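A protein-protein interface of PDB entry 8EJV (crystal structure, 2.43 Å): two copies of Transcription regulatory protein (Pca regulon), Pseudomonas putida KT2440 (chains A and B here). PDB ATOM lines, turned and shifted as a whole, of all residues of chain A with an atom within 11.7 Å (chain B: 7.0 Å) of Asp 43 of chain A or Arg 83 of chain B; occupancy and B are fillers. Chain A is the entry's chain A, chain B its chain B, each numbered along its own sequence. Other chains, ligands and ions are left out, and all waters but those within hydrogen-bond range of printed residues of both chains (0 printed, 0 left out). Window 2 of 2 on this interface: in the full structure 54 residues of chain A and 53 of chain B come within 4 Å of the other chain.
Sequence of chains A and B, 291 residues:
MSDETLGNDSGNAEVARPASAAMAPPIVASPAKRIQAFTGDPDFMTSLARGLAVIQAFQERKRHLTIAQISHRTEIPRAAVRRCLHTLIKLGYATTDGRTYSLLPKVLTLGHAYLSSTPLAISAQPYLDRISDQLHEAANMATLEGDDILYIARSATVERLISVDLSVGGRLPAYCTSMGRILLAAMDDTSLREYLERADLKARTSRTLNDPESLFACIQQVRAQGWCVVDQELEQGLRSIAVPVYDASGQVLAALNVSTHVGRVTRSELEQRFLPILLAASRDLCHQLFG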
ATOM      1  N   ILE A  35      -5.303  10.560   1.731  1.00  0.00           N
ATOM      2  CA  ILE A  35      -4.906  11.198   2.987  1.00  0.00           C
ATOM      3  C   ILE A  35      -5.911  10.876   4.090  1.00  0.00           C
ATOM      4  O   ILE A  35      -5.542  10.495   5.209  1.00  0.00           O
ATOM      5  CB  ILE A  35      -4.740  12.717   2.795  1.00  0.00           C
ATOM      6  CG1 ILE A  35      -3.538  13.018   1.894  1.00  0.00           C
ATOM      7  CG2 ILE A  35      -4.621  13.407   4.148  1.00  0.00           C
ATOM      8  CD1 ILE A  35      -3.719  14.220   0.999  1.00  0.00           C
ATOM      9  N   ALA A  37      -7.773   8.439   4.472  1.00  0.00           N
ATOM     10  CA  ALA A  37      -7.782   7.035   4.864  1.00  0.00           C
ATOM     11  C   ALA A  37      -6.910   6.766   6.078  1.00  0.00           C
ATOM     12  O   ALA A  37      -7.019   5.688   6.666  1.00  0.00           O
ATOM     13  CB  ALA A  37      -7.326   6.158   3.697  1.00  0.00           C
ATOM     14  N   PHE A  38      -6.042   7.706   6.457  1.00  0.00           N
ATOM     15  CA  PHE A  38      -5.218   7.560   7.648  1.00  0.00           C
ATOM     16  C   PHE A  38      -5.717   8.428   8.796  1.00  0.00           C
ATOM     17  O   PHE A  38      -5.005   8.594   9.788  1.00  0.00           O
ATOM     18  CB  PHE A  38      -3.753   7.890   7.346  1.00  0.00           C
ATOM     19  CG  PHE A  38      -3.136   7.048   6.253  1.00  0.00           C
ATOM     20  CD1 PHE A  38      -2.525   5.837   6.557  1.00  0.00           C
ATOM     21  CD2 PHE A  38      -3.178   7.461   4.928  1.00  0.00           C
ATOM     22  CE1 PHE A  38      -1.958   5.055   5.557  1.00  0.00           C
ATOM     23  CE2 PHE A  38      -2.608   6.690   3.924  1.00  0.00           C
ATOM     24  CZ  PHE A  38      -2.001   5.481   4.239  1.00  0.00           C
ATOM     25  N   THR A  39      -6.930   8.981   8.686  1.00  0.00           N
ATOM     26  CA  THR A  39      -7.383   9.948   9.680  1.00  0.00           C
ATOM     27  C   THR A  39      -7.506   9.328  11.068  1.00  0.00           C
ATOM     28  O   THR A  39      -7.556  10.063  12.061  1.00  0.00           O
ATOM     29  CB  THR A  39      -8.719  10.571   9.259  1.00  0.00           C
ATOM     30  OG1 THR A  39      -9.091  11.592  10.193  1.00  0.00           O
ATOM     31  CG2 THR A  39      -9.817   9.516   9.242  1.00  0.00           C
ATOM     32  N   GLY A  40      -7.540   7.996  11.160  1.00  0.00           N
ATOM     33  CA  GLY A  40      -7.527   7.311  12.439  1.00  0.00           C
ATOM     34  C   GLY A  40      -6.155   7.053  13.009  1.00  0.00           C
ATOM     35  O   GLY A  40      -6.044   6.551  14.133  1.00  0.00           O
ATOM     36  N   ASP A  41      -5.105   7.381  12.261  1.00  0.00           N
ATOM     37  CA  ASP A  41      -3.740   7.190  12.737  1.00  0.00           C
ATOM     38  C   ASP A  41      -3.234   8.488  13.349  1.00  0.00           C
ATOM     39  O   ASP A  41      -3.171   9.505  12.644  1.00  0.00           O
ATOM     40  CB  ASP A  41      -2.825   6.770  11.596  1.00  0.00           C
ATOM     41  CG  ASP A  41      -1.394   6.539  12.046  1.00  0.00           C
ATOM     42  OD1 ASP A  41      -1.017   7.070  13.116  1.00  0.00           O
ATOM     43  OD2 ASP A  41      -0.668   5.795  11.360  1.00  0.00           O
ATOM     44  N   PRO A  42      -2.856   8.501  14.629  1.00  0.00           N
ATOM     45  CA  PRO A  42      -2.471   9.765  15.270  1.00  0.00           C
ATOM     46  C   PRO A  42      -1.096  10.272  14.872  1.00  0.00           C
ATOM     47  O   PRO A  42      -0.804  11.455  15.097  1.00  0.00           O
ATOM     48  CB  PRO A  42      -2.518   9.428  16.768  1.00  0.00           C
ATOM     49  CG  PRO A  42      -2.403   7.921  16.852  1.00  0.00           C
ATOM     50  CD  PRO A  42      -2.636   7.328  15.492  1.00  0.00           C
ATOM     51  N   ASP A  43      -0.250   9.427  14.285  1.00  0.00           N
ATOM     52  CA  ASP A  43       1.091   9.819  13.885  1.00  0.00           C
ATOM     53  C   ASP A  43       1.169  10.225  12.419  1.00  0.00           C
ATOM     54  O   ASP A  43       2.267  10.474  11.916  1.00  0.00           O
ATOM     55  CB  ASP A  43       2.080   8.683  14.153  1.00  0.00           C
ATOM     56  CG  ASP A  43       2.358   8.490  15.626  1.00  0.00           C
ATOM     57  OD1 ASP A  43       2.553   9.502  16.334  1.00  0.00           O
ATOM     58  OD2 ASP A  43       2.362   7.324  16.078  1.00  0.00           O
ATOM     59  N   PHE A  44       0.040  10.287  11.721  1.00  0.00           N
ATOM     60  CA  PHE A  44       0.017  10.601  10.298  1.00  0.00           C
ATOM     61  C   PHE A  44      -0.253  12.092  10.129  1.00  0.00           C
ATOM     62  O   PHE A  44      -1.352  12.564  10.436  1.00  0.00           O
ATOM     63  CB  PHE A  44      -1.037   9.770   9.571  1.00  0.00           C
ATOM     64  CG  PHE A  44      -1.085  10.032   8.098  1.00  0.00           C
ATOM     65  CD1 PHE A  44      -0.222   9.375   7.236  1.00  0.00           C
ATOM     66  CD2 PHE A  44      -1.973  10.959   7.576  1.00  0.00           C
ATOM     67  CE1 PHE A  44      -0.256   9.630   5.878  1.00  0.00           C
ATOM     68  CE2 PHE A  44      -2.009  11.218   6.221  1.00  0.00           C
ATOM     69  CZ  PHE A  44      -1.152  10.551   5.371  1.00  0.00           C
ATOM     70  N   MET A  45       0.748  12.828   9.637  1.00  0.00           N
ATOM     71  CA  MET A  45       0.657  14.278   9.432  1.00  0.00           C
ATOM     72  C   MET A  45      -0.186  14.585   8.202  1.00  0.00           C
ATOM     73  O   MET A  45       0.306  14.552   7.074  1.00  0.00           O
ATOM     74  CB  MET A  45       2.047  14.889   9.288  1.00  0.00           C
ATOM     75  CG  MET A  45       2.907  14.841  10.524  1.00  0.00           C
ATOM     76  SD  MET A  45       1.920  14.825  12.036  1.00  0.00           S
ATOM     77  CE  MET A  45       3.014  15.725  13.125  1.00  0.00           C
ATOM     78  N   THR A  46      -1.457  14.922   8.427  1.00  0.00           N
ATOM     79  CA  THR A  46      -2.353  15.243   7.320  1.00  0.00           C
ATOM     80  C   THR A  46      -1.856  16.453   6.532  1.00  0.00           C
ATOM     81  O   THR A  46      -1.958  16.484   5.299  1.00  0.00           O
ATOM     82  CB  THR A  46      -3.770  15.479   7.854  1.00  0.00           C
ATOM     83  OG1 THR A  46      -4.331  14.231   8.290  1.00  0.00           O
ATOM     84  CG2 THR A  46      -4.667  16.075   6.787  1.00  0.00           C
ATOM     85  N   SER A  47      -1.299  17.459   7.215  1.00  0.00           N
ATOM     86  CA  SER A  47      -0.859  18.649   6.495  1.00  0.00           C
ATOM     87  C   SER A  47       0.432  18.393   5.726  1.00  0.00           C
ATOM     88  O   SER A  47       0.663  19.009   4.685  1.00  0.00           O
ATOM     89  CB  SER A  47      -0.711  19.832   7.460  1.00  0.00           C
ATOM     90  OG  SER A  47       0.434  19.719   8.298  1.00  0.00           O
ATOM     91  N   LEU A  48       1.273  17.471   6.189  1.00  0.00           N
ATOM     92  CA  LEU A  48       2.437  17.116   5.389  1.00  0.00           C
ATOM     93  C   LEU A  48       2.027  16.286   4.173  1.00  0.00           C
ATOM     94  O   LEU A  48       2.528  16.511   3.063  1.00  0.00           O
ATOM     95  CB  LEU A  48       3.464  16.380   6.251  1.00  0.00           C
ATOM     96  CG  LEU A  48       4.509  15.526   5.519  1.00  0.00           C
ATOM     97  CD1 LEU A  48       5.520  16.457   4.864  1.00  0.00           C
ATOM     98  CD2 LEU A  48       5.222  14.565   6.476  1.00  0.00           C
ATOM     99  N   ALA A  49       1.099  15.343   4.356  1.00  0.00           N
ATOM    100  CA  ALA A  49       0.545  14.614   3.220  1.00  0.00           C
ATOM    101  C   ALA A  49      -0.104  15.560   2.216  1.00  0.00           C
ATOM    102  O   ALA A  49       0.117  15.442   1.004  1.00  0.00           O
ATOM    103  CB  ALA A  49      -0.467  13.580   3.707  1.00  0.00           C
ATOM    104  N   ARG A  50      -0.903  16.513   2.701  1.00  0.00           N
ATOM    105  CA  ARG A  50      -1.537  17.471   1.799  1.00  0.00           C
ATOM    106  C   ARG A  50      -0.499  18.318   1.073  1.00  0.00           C
ATOM    107  O   ARG A  50      -0.601  18.538  -0.142  1.00  0.00           O
ATOM    108  CB  ARG A  50      -2.490  18.378   2.571  1.00  0.00           C
ATOM    109  CG  ARG A  50      -3.888  17.814   2.696  1.00  0.00           C
ATOM    110  CD  ARG A  50      -4.545  18.226   3.997  1.00  0.00           C
ATOM    111  NE  ARG A  50      -5.970  17.953   3.941  1.00  0.00           N
ATOM    112  CZ  ARG A  50      -6.885  18.547   4.693  1.00  0.00           C
ATOM    113  NH1 ARG A  50      -6.574  19.554   5.498  1.00  0.00           N
ATOM    114  NH2 ARG A  50      -8.147  18.134   4.621  1.00  0.00           N
ATOM    115  N   LEU A  52       2.625  17.573   0.341  1.00  0.00           N
ATOM    116  CA  LEU A  52       3.238  16.757  -0.703  1.00  0.00           C
ATOM    117  C   LEU A  52       2.276  16.531  -1.864  1.00  0.00           C
ATOM    118  O   LEU A  52       2.679  16.593  -3.036  1.00  0.00           O
ATOM    119  CB  LEU A  52       3.708  15.420  -0.138  1.00  0.00           C
ATOM    120  CG  LEU A  52       4.857  15.542   0.854  1.00  0.00           C
ATOM    121  CD1 LEU A  52       4.767  14.423   1.887  1.00  0.00           C
ATOM    122  CD2 LEU A  52       6.182  15.550   0.123  1.00  0.00           C
ATOM    123  N   SER B  47       4.275  20.835  10.486  1.00  0.00           N
ATOM    124  CA  SER B  47       4.582  19.451  10.136  1.00  0.00           C
ATOM    125  C   SER B  47       4.927  19.295   8.659  1.00  0.00           C
ATOM    126  O   SER B  47       5.659  18.367   8.284  1.00  0.00           O
ATOM    127  CB  SER B  47       3.404  18.554  10.505  1.00  0.00           C
ATOM    128  OG  SER B  47       2.293  18.849   9.682  1.00  0.00           O
ATOM    129  N   ARG B  50       8.581  20.441   8.577  1.00  0.00           N
ATOM    130  CA  ARG B  50       9.439  19.426   9.172  1.00  0.00           C
ATOM    131  C   ARG B  50       9.579  18.220   8.258  1.00  0.00           C
ATOM    132  O   ARG B  50      10.682  17.686   8.094  1.00  0.00           O
ATOM    133  CB  ARG B  50       8.880  19.020  10.532  1.00  0.00           C
ATOM    134  CG  ARG B  50       8.908  20.161  11.532  1.00  0.00           C
ATOM    135  CD  ARG B  50       8.481  19.708  12.892  1.00  0.00           C
ATOM    136  NE  ARG B  50       8.732  20.726  13.900  1.00  0.00           N
ATOM    137  CZ  ARG B  50       8.034  20.843  15.018  1.00  0.00           C
ATOM    138  NH1 ARG B  50       7.030  20.023  15.289  1.00  0.00           N
ATOM    139  NH2 ARG B  50       8.349  21.805  15.883  1.00  0.00           N
ATOM    140  N   ILE B  67      16.461   8.285  13.767  1.00  0.00           N
ATOM    141  CA  ILE B  67      15.761   9.438  14.324  1.00  0.00           C
ATOM    142  C   ILE B  67      16.766  10.414  14.914  1.00  0.00           C
ATOM    143  O   ILE B  67      16.679  11.629  14.699  1.00  0.00           O
ATOM    144  CB  ILE B  67      14.744   8.987  15.389  1.00  0.00           C
ATOM    145  CG1 ILE B  67      13.666   8.090  14.776  1.00  0.00           C
ATOM    146  CG2 ILE B  67      14.131  10.199  16.099  1.00  0.00           C
ATOM    147  CD1 ILE B  67      12.563   8.840  14.098  1.00  0.00           C
ATOM    148  N   PRO B  77      12.580  18.257  16.807  1.00  0.00           N
ATOM    149  CA  PRO B  77      12.468  17.331  17.944  1.00  0.00           C
ATOM    150  C   PRO B  77      12.197  15.906  17.480  1.00  0.00           C
ATOM    151  O   PRO B  77      11.528  15.671  16.471  1.00  0.00           O
ATOM    152  CB  PRO B  77      11.287  17.883  18.757  1.00  0.00           C
ATOM    153  CG  PRO B  77      10.793  19.098  18.035  1.00  0.00           C
ATOM    154  CD  PRO B  77      11.784  19.481  16.991  1.00  0.00           C
ATOM    155  N   ARG B  78      12.726  14.953  18.253  1.00  0.00           N
ATOM    156  CA  ARG B  78      12.692  13.543  17.863  1.00  0.00           C
ATOM    157  C   ARG B  78      11.271  13.049  17.621  1.00  0.00           C
ATOM    158  O   ARG B  78      11.018  12.335  16.643  1.00  0.00           O
ATOM    159  CB  ARG B  78      13.389  12.692  18.928  1.00  0.00           C
ATOM    160  CG  ARG B  78      14.916  12.742  18.815  1.00  0.00           C
ATOM    161  CD  ARG B  78      15.618  12.194  20.042  1.00  0.00           C
ATOM    162  NE  ARG B  78      17.064  12.391  19.988  1.00  0.00           N
ATOM    163  CZ  ARG B  78      17.959  11.458  20.287  1.00  0.00           C
ATOM    164  NH1 ARG B  78      17.593  10.235  20.634  1.00  0.00           N
ATOM    165  NH2 ARG B  78      19.254  11.762  20.248  1.00  0.00           N
ATOM    166  N   ALA B  79      10.326  13.421  18.486  1.00  0.00           N
ATOM    167  CA  ALA B  79       8.963  12.928  18.316  1.00  0.00           C
ATOM    168  C   ALA B  79       8.363  13.412  17.001  1.00  0.00           C
ATOM    169  O   ALA B  79       7.664  12.654  16.314  1.00  0.00           O
ATOM    170  CB  ALA B  79       8.085  13.347  19.496  1.00  0.00           C
ATOM    171  N   ALA B  80       8.635  14.665  16.624  1.00  0.00           N
ATOM    172  CA  ALA B  80       8.109  15.177  15.362  1.00  0.00           C
ATOM    173  C   ALA B  80       8.778  14.501  14.172  1.00  0.00           C
ATOM    174  O   ALA B  80       8.118  14.212  13.166  1.00  0.00           O
ATOM    175  CB  ALA B  80       8.287  16.693  15.284  1.00  0.00           C
ATOM    176  N   VAL B  81      10.088  14.240  14.269  1.00  0.00           N
ATOM    177  CA  VAL B  81      10.782  13.505  13.211  1.00  0.00           C
ATOM    178  C   VAL B  81      10.150  12.133  13.031  1.00  0.00           C
ATOM    179  O   VAL B  81       9.843  11.718  11.905  1.00  0.00           O
ATOM    180  CB  VAL B  81      12.285  13.384  13.528  1.00  0.00           C
ATOM    181  CG1 VAL B  81      12.916  12.306  12.659  1.00  0.00           C
ATOM    182  CG2 VAL B  81      12.988  14.713  13.340  1.00  0.00           C
ATOM    183  N   ARG B  82       9.931  11.420  14.144  1.00  0.00           N
ATOM    184  CA  ARG B  82       9.262  10.123  14.110  1.00  0.00           C
ATOM    185  C   ARG B  82       7.955  10.190  13.329  1.00  0.00           C
ATOM    186  O   ARG B  82       7.719   9.382  12.424  1.00  0.00           O
ATOM    187  CB  ARG B  82       9.012   9.625  15.543  1.00  0.00           C
ATOM    188  CG  ARG B  82       9.116   8.098  15.704  1.00  0.00           C
ATOM    189  CD  ARG B  82       9.172   7.650  17.173  1.00  0.00           C
ATOM    190  NE  ARG B  82      10.416   8.057  17.822  1.00  0.00           N
ATOM    191  CZ  ARG B  82      11.411   7.238  18.142  1.00  0.00           C
ATOM    192  NH1 ARG B  82      11.360   5.944  17.865  1.00  0.00           N
ATOM    193  NH2 ARG B  82      12.495   7.736  18.739  1.00  0.00           N
ATOM    194  N   ARG B  83       7.103  11.165  13.648  1.00  0.00           N
ATOM    195  CA  ARG B  83       5.808  11.257  12.979  1.00  0.00           C
ATOM    196  C   ARG B  83       5.963  11.623  11.507  1.00  0.00           C
ATOM    197  O   ARG B  83       5.242  11.090  10.648  1.00  0.00           O
ATOM    198  CB  ARG B  83       4.913  12.257  13.710  1.00  0.00           C
ATOM    199  CG  ARG B  83       4.531  11.762  15.104  1.00  0.00           C
ATOM    200  CD  ARG B  83       3.858  12.804  15.991  1.00  0.00           C
ATOM    201  NE  ARG B  83       4.153  14.176  15.604  1.00  0.00           N
ATOM    202  CZ  ARG B  83       4.483  15.136  16.457  1.00  0.00           C
ATOM    203  NH1 ARG B  83       4.607  14.897  17.752  1.00  0.00           N
ATOM    204  NH2 ARG B  83       4.704  16.364  15.999  1.00  0.00           N
ATOM    205  N   CYS B  84       6.907  12.516  11.195  1.00  0.00           N
ATOM    206  CA  CYS B  84       7.170  12.871   9.803  1.00  0.00           C
ATOM    207  C   CYS B  84       7.592  11.651   8.998  1.00  0.00           C
ATOM    208  O   CYS B  84       7.043  11.381   7.923  1.00  0.00           O
ATOM    209  CB  CYS B  84       8.248  13.951   9.736  1.00  0.00           C
ATOM    210  SG  CYS B  84       7.647  15.582  10.183  1.00  0.00           S
ATOM    211  N   LEU B  85       8.573  10.899   9.504  1.00  0.00           N
ATOM    212  CA  LEU B  85       9.008   9.691   8.806  1.00  0.00           C
ATOM    213  C   LEU B  85       7.857   8.705   8.641  1.00  0.00           C
ATOM    214  O   LEU B  85       7.665   8.136   7.559  1.00  0.00           O
ATOM    215  CB  LEU B  85      10.165   9.037   9.558  1.00  0.00           C
ATOM    216  CG  LEU B  85      11.484   9.775   9.384  1.00  0.00           C
ATOM    217  CD1 LEU B  85      12.435   9.390  10.488  1.00  0.00           C
ATOM    218  CD2 LEU B  85      12.089   9.484   8.008  1.00  0.00           C
ATOM    219  N   HIS B  86       7.076   8.499   9.705  1.00  0.00           N
ATOM    220  CA  HIS B  86       5.921   7.609   9.626  1.00  0.00           C
ATOM    221  C   HIS B  86       4.989   8.019   8.493  1.00  0.00           C
ATOM    222  O   HIS B  86       4.520   7.171   7.725  1.00  0.00           O
ATOM    223  CB  HIS B  86       5.174   7.608  10.964  1.00  0.00           C
ATOM    224  CG  HIS B  86       3.972   6.719  10.992  1.00  0.00           C
ATOM    225  ND1 HIS B  86       4.063   5.359  11.195  1.00  0.00           N
ATOM    226  CD2 HIS B  86       2.651   6.992  10.867  1.00  0.00           C
ATOM    227  CE1 HIS B  86       2.853   4.830  11.183  1.00  0.00           C
ATOM    228  NE2 HIS B  86       1.977   5.800  10.985  1.00  0.00           N
ATOM    229  N   THR B  87       4.716   9.318   8.375  1.00  0.00           N
ATOM    230  CA  THR B  87       3.866   9.804   7.296  1.00  0.00           C
ATOM    231  C   THR B  87       4.507   9.564   5.937  1.00  0.00           C
ATOM    232  O   THR B  87       3.830   9.147   4.991  1.00  0.00           O
ATOM    233  CB  THR B  87       3.571  11.287   7.508  1.00  0.00           C
ATOM    234  OG1 THR B  87       2.922  11.460   8.776  1.00  0.00           O
ATOM    235  CG2 THR B  87       2.700  11.835   6.388  1.00  0.00           C
ATOM    236  N   LEU B  88       5.814   9.809   5.825  1.00  0.00           N
ATOM    237  CA  LEU B  88       6.505   9.571   4.564  1.00  0.00           C
ATOM    238  C   LEU B  88       6.477   8.100   4.183  1.00  0.00           C
ATOM    239  O   LEU B  88       6.316   7.760   3.003  1.00  0.00           O
ATOM    240  CB  LEU B  88       7.948  10.065   4.645  1.00  0.00           C
ATOM    241  CG  LEU B  88       8.106  11.583   4.731  1.00  0.00           C
ATOM    242  CD1 LEU B  88       9.536  11.985   5.109  1.00  0.00           C
ATOM    243  CD2 LEU B  88       7.669  12.222   3.416  1.00  0.00           C
ATOM    244  N   ILE B  89       6.646   7.208   5.164  1.00  0.00           N
ATOM    245  CA  ILE B  89       6.569   5.779   4.881  1.00  0.00           C
ATOM    246  C   ILE B  89       5.180   5.406   4.378  1.00  0.00           C
ATOM    247  O   ILE B  89       5.034   4.726   3.356  1.00  0.00           O
ATOM    248  CB  ILE B  89       6.958   4.958   6.125  1.00  0.00           C
ATOM    249  CG1 ILE B  89       8.468   5.001   6.332  1.00  0.00           C
ATOM    250  CG2 ILE B  89       6.440   3.531   6.015  1.00  0.00           C
ATOM    251  CD1 ILE B  89       8.871   4.898   7.788  1.00  0.00           C
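The side-chain hydroxyl (OG1) of Thr 87 of chain B sits at hydrogen-bond distance from the backbone NH (N) of Met 45 of chain A, 2.7 Å away.
The side-chain hydroxyl (OG) of Ser 47 of chain B is in hydrogen-bond range of the side-chain hydroxyl (OG) of Ser 47 of chain A.
The side-chain carboxylate (OD2) of Asp 41 of chain A sits at hydrogen-bond distance from a ring nitrogen (NE2) of His 86 of chain B (2.7 Å).
OG1 of Thr 87 of chain B lies within hydrogen-bond range of O of Asp 43 of chain A (3.4 Å).
The backbone carbonyl oxygen of Asp 43 of chain A lies close to the backbone carbonyl oxygen of Arg 83 of chain B (3.3 Å).
The side-chain carboxylate (OD1) of Asp 41 of chain A is in hydrogen-bond range of the backbone NH (N) of Asp 43 of chain A.
The backbone carbonyl oxygen of Arg 83 of chain B is in hydrogen-bond range of the side-chain hydroxyl of Thr 87 of chain B.
O of Ala 80 of chain B sits at hydrogen-bond distance from SG of Cys 84 of chain B, 3.3 Å away.
Among the printed residues, pairs that only touch across the chains: Asp 43 of chain A with His 86 of chain B, Phe 44 of chain A with Thr 87 of chain B, Met 45 of chain A with Ser 47 of chain B, Met 45 of chain A with Arg 83 of chain B, Leu 48 of chain A with Ser 47 of chain B, Leu 48 of chain A with Cys 84 of chain B, Leu 48 of chain A with Thr 87 of chain B and Leu 52 of chain A with Leu 88 of chain B.
Of chain B, only Arg 83, His 86 and Thr 87 come within 4 Å of Asp 43 of chain A.
Of the printed residues of chain B, Phe 44 of chain A touches Thr 87 (3.4 Å).
Of the printed residues of chain B, Met 45 of chain A touches Ser 47 (3.7 Å), Arg 83 (3.1 Å) and Thr 87 (2.7 Å).
Of chain A, only Asp 43 (3.2 Å) and Met 45 (3.1 Å) come within 4 Å of Arg 83 of chain B.
Of chain A, only Leu 48 comes within 4 Å of Cys 84 of chain B.
No residue of chain A comes within 4 Å of Leu 85 of chain B.
His 86 of chain B touches just these residues of chain A: Asp 41 and Asp 43.
Thr 87 of chain B touches just these residues of chain A: Asp 43 (3.4 Å), Phe 44 (3.4 Å), Met 45 (2.7 Å) and Leu 48 (3.7 Å).
Ile 89 of chain B touches none of the printed residues of chain A.
The nearest residue of chain B that does not touch Asp 43 of chain A is Cys 84 of chain B (5.1 Å).
The nearest residue of chain A that does not touch Arg 83 of chain B is Pro 42 of chain A (4.9 Å).
The nearest printed residue of chain B that does not touch Asp 41 of chain A is Thr 87 of chain B (7.1 Å).
Of the 16 printed residues of chain A, 7 touch a printed residue of chain B.
Hydrophobic or aromatic side chains of chain A that line the printed part of chain B: Phe 44, Met 45, Leu 48 and Leu 52.
Along chain A the printed residues that touch a printed residue of chain B span positions 41 to 52.
Of the 16 printed residues of chain B, 6 touch a printed residue of chain A.
Ser 47 of chain A touches its own counterpart, Ser 47 of chain B.
2 positions are printed for both chains.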
